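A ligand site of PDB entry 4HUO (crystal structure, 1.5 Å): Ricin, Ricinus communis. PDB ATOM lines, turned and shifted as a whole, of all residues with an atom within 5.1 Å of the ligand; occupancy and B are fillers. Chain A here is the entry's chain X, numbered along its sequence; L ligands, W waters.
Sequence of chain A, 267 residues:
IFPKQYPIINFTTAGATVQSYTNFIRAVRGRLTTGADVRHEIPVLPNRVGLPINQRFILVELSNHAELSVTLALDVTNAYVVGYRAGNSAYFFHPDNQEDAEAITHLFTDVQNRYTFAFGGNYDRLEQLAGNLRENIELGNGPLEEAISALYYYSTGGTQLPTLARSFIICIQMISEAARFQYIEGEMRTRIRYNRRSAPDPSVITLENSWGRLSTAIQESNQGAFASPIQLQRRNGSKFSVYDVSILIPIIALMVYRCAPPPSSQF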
ATOM      1  N   ASN A  78       5.468  33.920  -5.469  1.00  0.00           N
ATOM      2  CA  ASN A  78       4.458  32.795  -5.496  1.00  0.00           C
ATOM      3  C   ASN A  78       4.764  31.794  -4.390  1.00  0.00           C
ATOM      4  O   ASN A  78       4.086  30.779  -4.324  1.00  0.00           O
ATOM      5  CB  ASN A  78       4.433  32.116  -6.872  1.00  0.00           C
ATOM      6  CG  ASN A  78       5.823  31.664  -7.327  1.00  0.00           C
ATOM      7  OD1 ASN A  78       6.826  31.751  -6.588  1.00  0.00           O
ATOM      8  ND2 ASN A  78       5.931  31.356  -8.651  1.00  0.00           N
ATOM      9  N   ALA A  79       5.792  32.038  -3.590  1.00  0.00           N
ATOM     10  CA  ALA A  79       6.273  31.124  -2.507  1.00  0.00           C
ATOM     11  C   ALA A  79       6.782  29.774  -3.066  1.00  0.00           C
ATOM     12  O   ALA A  79       7.026  28.842  -2.333  1.00  0.00           O
ATOM     13  CB  ALA A  79       5.219  30.853  -1.403  1.00  0.00           C
ATOM     14  N   TYR A  80       7.145  29.784  -4.338  1.00  0.00           N
ATOM     15  CA  TYR A  80       7.546  28.532  -5.019  1.00  0.00           C
ATOM     16  C   TYR A  80       8.979  28.183  -4.752  1.00  0.00           C
ATOM     17  O   TYR A  80       9.866  29.026  -4.610  1.00  0.00           O
ATOM     18  CB  TYR A  80       7.407  28.818  -6.506  1.00  0.00           C
ATOM     19  CG  TYR A  80       7.388  27.623  -7.395  1.00  0.00           C
ATOM     20  CD1 TYR A  80       8.584  27.085  -7.850  1.00  0.00           C
ATOM     21  CD2 TYR A  80       6.235  27.105  -7.788  1.00  0.00           C
ATOM     22  CE1 TYR A  80       8.573  26.006  -8.679  1.00  0.00           C
ATOM     23  CE2 TYR A  80       6.171  26.019  -8.603  1.00  0.00           C
ATOM     24  CZ  TYR A  80       7.376  25.456  -9.023  1.00  0.00           C
ATOM     25  OH  TYR A  80       7.424  24.367  -9.889  1.00  0.00           O
ATOM     26  N   VAL A  81       9.230  26.895  -4.445  1.00  0.00           N
ATOM     27  CA  VAL A  81      10.589  26.412  -4.146  1.00  0.00           C
ATOM     28  C   VAL A  81      11.273  26.270  -5.502  1.00  0.00           C
ATOM     29  O   VAL A  81      10.934  25.368  -6.293  1.00  0.00           O
ATOM     30  CB  VAL A  81      10.552  25.035  -3.478  1.00  0.00           C
ATOM     31  CG1 VAL A  81      12.021  24.523  -3.246  1.00  0.00           C
ATOM     32  CG2 VAL A  81       9.762  25.136  -2.101  1.00  0.00           C
ATOM     33  N   PHE A  93      15.139  23.789 -10.325  1.00  0.00           N
ATOM     34  CA  PHE A  93      14.196  23.236 -11.231  1.00  0.00           C
ATOM     35  C   PHE A  93      14.330  24.014 -12.581  1.00  0.00           C
ATOM     36  O   PHE A  93      14.831  25.158 -12.584  1.00  0.00           O
ATOM     37  CB  PHE A  93      12.743  23.255 -10.721  1.00  0.00           C
ATOM     38  CG  PHE A  93      12.558  22.515  -9.481  1.00  0.00           C
ATOM     39  CD1 PHE A  93      12.655  21.120  -9.516  1.00  0.00           C
ATOM     40  CD2 PHE A  93      12.351  23.153  -8.275  1.00  0.00           C
ATOM     41  CE1 PHE A  93      12.483  20.353  -8.375  1.00  0.00           C
ATOM     42  CE2 PHE A  93      12.155  22.399  -7.092  1.00  0.00           C
ATOM     43  CZ  PHE A  93      12.243  20.984  -7.132  1.00  0.00           C
ATOM     44  N   GLY A 121       9.531  21.923 -11.614  1.00  0.00           N
ATOM     45  CA  GLY A 121       9.313  21.578 -10.190  1.00  0.00           C
ATOM     46  C   GLY A 121       7.837  21.498  -9.861  1.00  0.00           C
ATOM     47  O   GLY A 121       7.545  21.372  -8.641  1.00  0.00           O
ATOM     48  N   ASN A 122       6.893  21.466 -10.808  1.00  0.00           N
ATOM     49  CA  ASN A 122       5.480  21.318 -10.458  1.00  0.00           C
ATOM     50  C   ASN A 122       5.117  19.934  -9.919  1.00  0.00           C
ATOM     51  O   ASN A 122       5.824  18.928 -10.219  1.00  0.00           O
ATOM     52  CB  ASN A 122       4.538  21.726 -11.588  1.00  0.00           C
ATOM     53  CG  ASN A 122       4.532  23.194 -11.878  1.00  0.00           C
ATOM     54  OD1 ASN A 122       5.037  24.017 -11.119  1.00  0.00           O
ATOM     55  ND2 ASN A 122       3.943  23.537 -13.037  1.00  0.00           N
ATOM     56  N   TYR A 123       4.074  19.876  -9.115  1.00  0.00           N
ATOM     57  CA  TYR A 123       3.674  18.588  -8.536  1.00  0.00           C
ATOM     58  C   TYR A 123       3.481  17.493  -9.596  1.00  0.00           C
ATOM     59  O   TYR A 123       3.891  16.390  -9.351  1.00  0.00           O
ATOM     60  CB  TYR A 123       2.403  18.621  -7.703  1.00  0.00           C
ATOM     61  CG  TYR A 123       2.443  19.467  -6.472  1.00  0.00           C
ATOM     62  CD1 TYR A 123       3.473  19.303  -5.501  1.00  0.00           C
ATOM     63  CD2 TYR A 123       1.353  20.336  -6.205  1.00  0.00           C
ATOM     64  CE1 TYR A 123       3.480  20.074  -4.313  1.00  0.00           C
ATOM     65  CE2 TYR A 123       1.348  21.077  -4.983  1.00  0.00           C
ATOM     66  CZ  TYR A 123       2.455  20.956  -4.118  1.00  0.00           C
ATOM     67  OH  TYR A 123       2.412  21.635  -2.956  1.00  0.00           O
ATOM     68  N   ASP A 124       2.852  17.812 -10.734  1.00  0.00           N
ATOM     69  CA  ASP A 124       2.550  16.726 -11.679  1.00  0.00           C
ATOM     70  C   ASP A 124       3.884  16.024 -12.107  1.00  0.00           C
ATOM     71  O   ASP A 124       3.950  14.770 -12.112  1.00  0.00           O
ATOM     72  CB  ASP A 124       1.827  17.287 -12.935  1.00  0.00           C
ATOM     73  CG  ASP A 124       1.300  16.191 -13.855  1.00  0.00           C
ATOM     74  OD1 ASP A 124       1.482  14.968 -13.581  1.00  0.00           O
ATOM     75  OD2 ASP A 124       0.676  16.555 -14.910  1.00  0.00           O
ATOM     76  N   LEU A 126       6.804  16.136 -10.474  1.00  0.00           N
ATOM     77  CA  LEU A 126       7.470  15.478  -9.340  1.00  0.00           C
ATOM     78  C   LEU A 126       6.764  14.179  -8.942  1.00  0.00           C
ATOM     79  O   LEU A 126       7.487  13.224  -8.597  1.00  0.00           O
ATOM     80  CB  LEU A 126       7.436  16.477  -8.142  1.00  0.00           C
ATOM     81  CG  LEU A 126       8.411  17.687  -8.357  1.00  0.00           C
ATOM     82  CD1 LEU A 126       8.242  18.546  -7.083  1.00  0.00           C
ATOM     83  CD2 LEU A 126       9.954  17.441  -8.602  1.00  0.00           C
ATOM     84  N   ARG A 134       0.629  12.959  -4.580  1.00  0.00           N
ATOM     85  CA  ARG A 134       0.514  13.607  -3.268  1.00  0.00           C
ATOM     86  C   ARG A 134      -0.343  12.848  -2.291  1.00  0.00           C
ATOM     87  O   ARG A 134      -0.030  12.700  -1.094  1.00  0.00           O
ATOM     88  CB  ARG A 134      -0.034  15.042  -3.427  1.00  0.00           C
ATOM     89  CG  ARG A 134       1.078  15.963  -3.759  1.00  0.00           C
ATOM     90  CD  ARG A 134       0.448  17.343  -4.105  1.00  0.00           C
ATOM     91  NE  ARG A 134      -0.229  17.294  -5.451  1.00  0.00           N
ATOM     92  CZ  ARG A 134      -1.150  18.120  -5.890  1.00  0.00           C
ATOM     93  NH1 ARG A 134      -1.589  19.141  -5.123  1.00  0.00           N
ATOM     94  NH2 ARG A 134      -1.570  18.002  -7.163  1.00  0.00           N
ATOM     95  N   ILE A 172       7.779  21.028  -0.136  1.00  0.00           N
ATOM     96  CA  ILE A 172       6.921  22.099  -0.695  1.00  0.00           C
ATOM     97  C   ILE A 172       5.655  22.190   0.142  1.00  0.00           C
ATOM     98  O   ILE A 172       5.199  23.290   0.450  1.00  0.00           O
ATOM     99  CB  ILE A 172       6.675  21.798  -2.138  1.00  0.00           C
ATOM    100  CG1 ILE A 172       7.971  21.843  -3.002  1.00  0.00           C
ATOM    101  CG2 ILE A 172       5.521  22.682  -2.795  1.00  0.00           C
ATOM    102  CD1 ILE A 172       7.799  21.029  -4.405  1.00  0.00           C
ATOM    103  N   SER A 176       5.929  25.757   1.607  1.00  0.00           N
ATOM    104  CA  SER A 176       5.208  26.704   0.795  1.00  0.00           C
ATOM    105  C   SER A 176       3.694  26.614   0.972  1.00  0.00           C
ATOM    106  O   SER A 176       2.987  27.652   1.052  1.00  0.00           O
ATOM    107  CB  SER A 176       5.557  26.511  -0.714  1.00  0.00           C
ATOM    108  OG  SER A 176       6.970  26.582  -0.813  1.00  0.00           O
ATOM    109  N   GLU A 177       3.113  25.420   0.933  1.00  0.00           N
ATOM    110  CA  GLU A 177       1.657  25.318   1.083  1.00  0.00           C
ATOM    111  C   GLU A 177       1.181  25.743   2.437  1.00  0.00           C
ATOM    112  O   GLU A 177       0.072  26.389   2.576  1.00  0.00           O
ATOM    113  CB  GLU A 177       1.105  23.899   0.766  1.00  0.00           C
ATOM    114  CG  GLU A 177       1.459  23.440  -0.620  1.00  0.00           C
ATOM    115  CD  GLU A 177       0.692  24.147  -1.773  1.00  0.00           C
ATOM    116  OE1 GLU A 177       0.053  25.230  -1.603  1.00  0.00           O
ATOM    117  OE2 GLU A 177       0.839  23.607  -2.911  1.00  0.00           O
ATOM    118  N   ARG A 180       1.082  29.431   2.360  1.00  0.00           N
ATOM    119  CA  ARG A 180      -0.025  29.942   1.547  1.00  0.00           C
ATOM    120  C   ARG A 180      -1.387  29.824   2.344  1.00  0.00           C
ATOM    121  O   ARG A 180      -2.299  30.651   2.134  1.00  0.00           O
ATOM    122  CB  ARG A 180      -0.084  29.199   0.235  1.00  0.00           C
ATOM    123  CG  ARG A 180       0.998  29.557  -0.762  1.00  0.00           C
ATOM    124  CD  ARG A 180       0.946  28.550  -1.868  1.00  0.00           C
ATOM    125  NE  ARG A 180       2.133  28.714  -2.735  1.00  0.00           N
ATOM    126  CZ  ARG A 180       2.793  27.721  -3.305  1.00  0.00           C
ATOM    127  NH1 ARG A 180       2.410  26.447  -3.084  1.00  0.00           N
ATOM    128  NH2 ARG A 180       3.869  28.001  -4.074  1.00  0.00           N
ATOM    129  N   GLU A 208      -4.547  23.171  -2.385  1.00  0.00           N
ATOM    130  CA  GLU A 208      -3.328  23.307  -3.152  1.00  0.00           C
ATOM    131  C   GLU A 208      -3.589  23.552  -4.610  1.00  0.00           C
ATOM    132  O   GLU A 208      -3.043  24.462  -5.181  1.00  0.00           O
ATOM    133  CB  GLU A 208      -2.408  22.077  -3.028  1.00  0.00           C
ATOM    134  CG  GLU A 208      -2.057  21.761  -1.546  1.00  0.00           C
ATOM    135  CD  GLU A 208      -1.212  20.570  -1.410  1.00  0.00           C
ATOM    136  OE1 GLU A 208      -1.126  19.701  -2.292  1.00  0.00           O
ATOM    137  OE2 GLU A 208      -0.673  20.301  -0.238  1.00  0.00           O
ATOM    138  N   ASN A 209      -4.474  22.710  -5.197  1.00  0.00           N
ATOM    139  CA  ASN A 209      -4.665  22.811  -6.631  1.00  0.00           C
ATOM    140  C   ASN A 209      -5.422  24.058  -6.992  1.00  0.00           C
ATOM    141  O   ASN A 209      -5.346  24.469  -8.167  1.00  0.00           O
ATOM    142  CB  ASN A 209      -5.468  21.588  -7.124  1.00  0.00           C
ATOM    143  CG  ASN A 209      -4.629  20.315  -7.009  1.00  0.00           C
ATOM    144  OD1 ASN A 209      -3.374  20.383  -7.013  1.00  0.00           O
ATOM    145  ND2 ASN A 209      -5.308  19.187  -7.073  1.00  0.00           N
ATOM    146  N   TRP A 211      -5.149  27.164  -5.462  1.00  0.00           N
ATOM    147  CA  TRP A 211      -4.620  28.442  -4.953  1.00  0.00           C
ATOM    148  C   TRP A 211      -4.679  29.551  -5.986  1.00  0.00           C
ATOM    149  O   TRP A 211      -4.977  30.702  -5.638  1.00  0.00           O
ATOM    150  CB  TRP A 211      -3.183  28.237  -4.476  1.00  0.00           C
ATOM    151  CG  TRP A 211      -2.592  29.479  -3.814  1.00  0.00           C
ATOM    152  CD1 TRP A 211      -3.117  30.083  -2.692  1.00  0.00           C
ATOM    153  CD2 TRP A 211      -1.365  30.095  -4.103  1.00  0.00           C
ATOM    154  NE1 TRP A 211      -2.281  31.157  -2.344  1.00  0.00           N
ATOM    155  CE2 TRP A 211      -1.218  31.149  -3.214  1.00  0.00           C
ATOM    156  CE3 TRP A 211      -0.421  29.903  -5.133  1.00  0.00           C
ATOM    157  CZ2 TRP A 211      -0.071  31.984  -3.210  1.00  0.00           C
ATOM    158  CZ3 TRP A 211       0.733  30.733  -5.141  1.00  0.00           C
ATOM    159  CH2 TRP A 211       0.866  31.766  -4.196  1.00  0.00           C
ATOM    160  N   GLY A 212      -4.243  29.280  -7.183  1.00  0.00           N
ATOM    161  CA  GLY A 212      -4.316  30.324  -8.212  1.00  0.00           C
ATOM    162  C   GLY A 212      -5.720  30.750  -8.560  1.00  0.00           C
ATOM    163  O   GLY A 212      -5.938  32.001  -8.697  1.00  0.00           O
ATOM    164  N   ARG A 258      -2.649  38.698  -8.979  1.00  0.00           N
ATOM    165  CA  ARG A 258      -3.283  38.347 -10.269  1.00  0.00           C
ATOM    166  C   ARG A 258      -3.868  39.539 -10.966  1.00  0.00           C
ATOM    167  O   ARG A 258      -3.844  39.596 -12.201  1.00  0.00           O
ATOM    168  CB  ARG A 258      -4.429  37.336 -10.067  1.00  0.00           C
ATOM    169  CG  ARG A 258      -3.967  35.974  -9.558  1.00  0.00           C
ATOM    170  CD  ARG A 258      -3.344  35.306 -10.748  1.00  0.00           C
ATOM    171  NE  ARG A 258      -2.889  33.925 -10.689  1.00  0.00           N
ATOM    172  CZ  ARG A 258      -1.643  33.571 -10.847  1.00  0.00           C
ATOM    173  NH1 ARG A 258      -0.683  34.491 -10.977  1.00  0.00           N
ATOM    174  NH2 ARG A 258      -1.327  32.273 -10.814  1.00  0.00           N
HETATM  175  C1  LIG L   1       7.454  23.810  -6.307  1.00  0.00           C
HETATM  176  N1  LIG L   1       8.701  23.424  -6.597  1.00  0.00           N
HETATM  177  O1  LIG L   1       5.834  25.919  -4.155  1.00  0.00           O
HETATM  178  C2  LIG L   1       6.021  25.061  -5.055  1.00  0.00           C
HETATM  179  N2  LIG L   1       7.251  24.722  -5.324  1.00  0.00           N
HETATM  180  C3  LIG L   1       4.892  24.451  -5.674  1.00  0.00           C
HETATM  181  N3  LIG L   1       6.481  23.123  -6.846  1.00  0.00           N
HETATM  182  O2  LIG L   1       2.150  22.083  -9.019  1.00  0.00           O
HETATM  183  C4  LIG L   1       5.206  23.501  -6.747  1.00  0.00           C
HETATM  184  N4  LIG L   1       4.212  22.877  -7.387  1.00  0.00           N
HETATM  185  C5  LIG L   1       2.973  23.282  -7.175  1.00  0.00           C
HETATM  186  N5  LIG L   1       3.626  24.828  -5.430  1.00  0.00           N
HETATM  187  C6  LIG L   1       2.674  24.222  -6.123  1.00  0.00           C
HETATM  188  C7  LIG L   1       1.849  22.706  -7.992  1.00  0.00           C
HETATM  189  N6  LIG L   1       0.610  23.079  -7.736  1.00  0.00           N
HETATM  190  C8  LIG L   1      -0.515  22.457  -8.430  1.00  0.00           C
HETATM  191  C9  LIG L   1      -1.449  23.520  -9.020  1.00  0.00           C
HETATM  192  O3  LIG L   1      -2.491  23.090  -9.453  1.00  0.00           O
HETATM  193  N7  LIG L   1      -1.008  24.794  -8.998  1.00  0.00           N
HETATM  194  C10 LIG L   1      -1.713  25.946  -9.583  1.00  0.00           C
HETATM  195  C11 LIG L   1      -1.065  26.249 -10.919  1.00  0.00           C
HETATM  196  O4  LIG L   1      -1.493  27.074 -11.718  1.00  0.00           O
HETATM  197  C12 LIG L   1      -1.815  27.015  -8.438  1.00  0.00           C
HETATM  198  C13 LIG L   1      -0.365  27.551  -8.153  1.00  0.00           C
HETATM  199  C14 LIG L   1       0.208  28.577  -8.910  1.00  0.00           C
HETATM  200  C15 LIG L   1       0.409  26.993  -7.159  1.00  0.00           C
HETATM  201  C16 LIG L   1       1.484  29.106  -8.687  1.00  0.00           C
HETATM  202  C17 LIG L   1       1.710  27.480  -6.954  1.00  0.00           C
HETATM  203  C18 LIG L   1       2.276  28.535  -7.674  1.00  0.00           C
HETATM  204  O5  LIG L   1       0.016  25.559 -11.289  1.00  0.00           O
HETATM  205  O   HOH W   1       2.623  25.535  -9.742  1.00  0.00           O
HETATM  206  O   HOH W   2       1.390  20.391 -11.110  1.00  0.00           O
HETATM  207  O   HOH W   3      -4.493  27.614 -11.508  1.00  0.00           O
HETATM  208  O   HOH W   4      -4.852  23.710 -11.005  1.00  0.00           O
HETATM  209  O   HOH W   5      -3.083  20.583 -10.438  1.00  0.00           O
HETATM  210  O   HOH W   6      -0.364  24.291  -5.275  1.00  0.00           O
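The backbone carbonyl oxygen (O) of Gly 121 sits at hydrogen-bond distance from a nitrogen (N1) of the ligand, 3.1 Å away.
An oxygen (O1) of the ligand is in hydrogen-bond range of the guanidinium group (NH2) of Arg 180, 2.9 Å away.
N of Tyr 123 sits at hydrogen-bond distance from O2 of the ligand (2.9 Å).
N of Val 81 is in hydrogen-bond range of N2 of the ligand (3.1 Å).
A nitrogen (N1) of the ligand sits at hydrogen-bond distance from the backbone carbonyl oxygen of Val 81, 3.0 Å away.
The side-chain hydroxyl of Tyr 80 sits close to a nitrogen (N3) of the ligand, at 3.4 Å.
The backbone carbonyl oxygen of Gly 121 lies close to the side-chain hydroxyl of Tyr 80, at 3.2 Å.
The side-chain carboxylate (OE1) of Glu 177 is in salt-bridge range of the guanidinium group (NH1) of Arg 180, at 3.0 Å.
NH2 of Arg 180 is in hydrogen-bond range of O of Asn 78 (2.8 Å).
OD1 of Asn 122 lies within hydrogen-bond range of OH of Tyr 80, 2.7 Å away.
N of Tyr 80 sits close to OD1 of Asn 78 (3.0 Å).
The backbone carbonyl oxygen (O) of Ile 172 sits at hydrogen-bond distance from the backbone NH (N) of Glu 177 (3.0 Å).
The side-chain amide oxygen (OD1) of Asn 209 is in hydrogen-bond range of the guanidinium group (NH1) of Arg 134 (2.9 Å).
OG of Ser 176 sits at hydrogen-bond distance from O of Ala 79 (2.7 Å).
The backbone carbonyl oxygen (O) of Asn 209 sits close to an oxygen (O3) of the ligand (3.4 Å).
Ala 79 touches the ligand.
Phe 93 touches the ligand (CE2 to N1, 3.6 Å).
Asn 122 touches the ligand (CB to O2, 3.5 Å).
CG2 of Ile 172 touches C2 of the ligand (3.3 Å).
Ser 176 touches the ligand.
Glu 177 touches the ligand.
Trp 211 touches the ligand (CE3 to C15, 3.6 Å).
Gly 212 touches the ligand.
Hydrophobic or aromatic side chains that line the ligand: Tyr 80, Val 81, Phe 93, Tyr 123, Ile 172 and Trp 211.
Along chain A the residues within 4 Å of the ligand span positions 79 to 212.
The nearest printed residue that does not touch the ligand is Asn 78 (4.3 Å).
Water W5 lies within hydrogen-bond range of O3 of the ligand (2.8 Å) and OD1 of Asn 209 (3.4 Å).
Water W2 lies within hydrogen-bond range of an oxygen (O2) of the ligand, the backbone NH of Asp 124 and the backbone NH of Tyr 123.
Water W4 lies within hydrogen-bond range of an oxygen (O3) of the ligand and the backbone carbonyl oxygen (O) of Asn 209.
Water W6 lies within hydrogen-bond range of O of Glu 208 (2.7 Å), OE2 of Glu 177 (2.7 Å) and N6 of the ligand (2.9 Å).
Water W1 lies within hydrogen-bond range of O5 of the ligand and OD1 of Asn 122.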
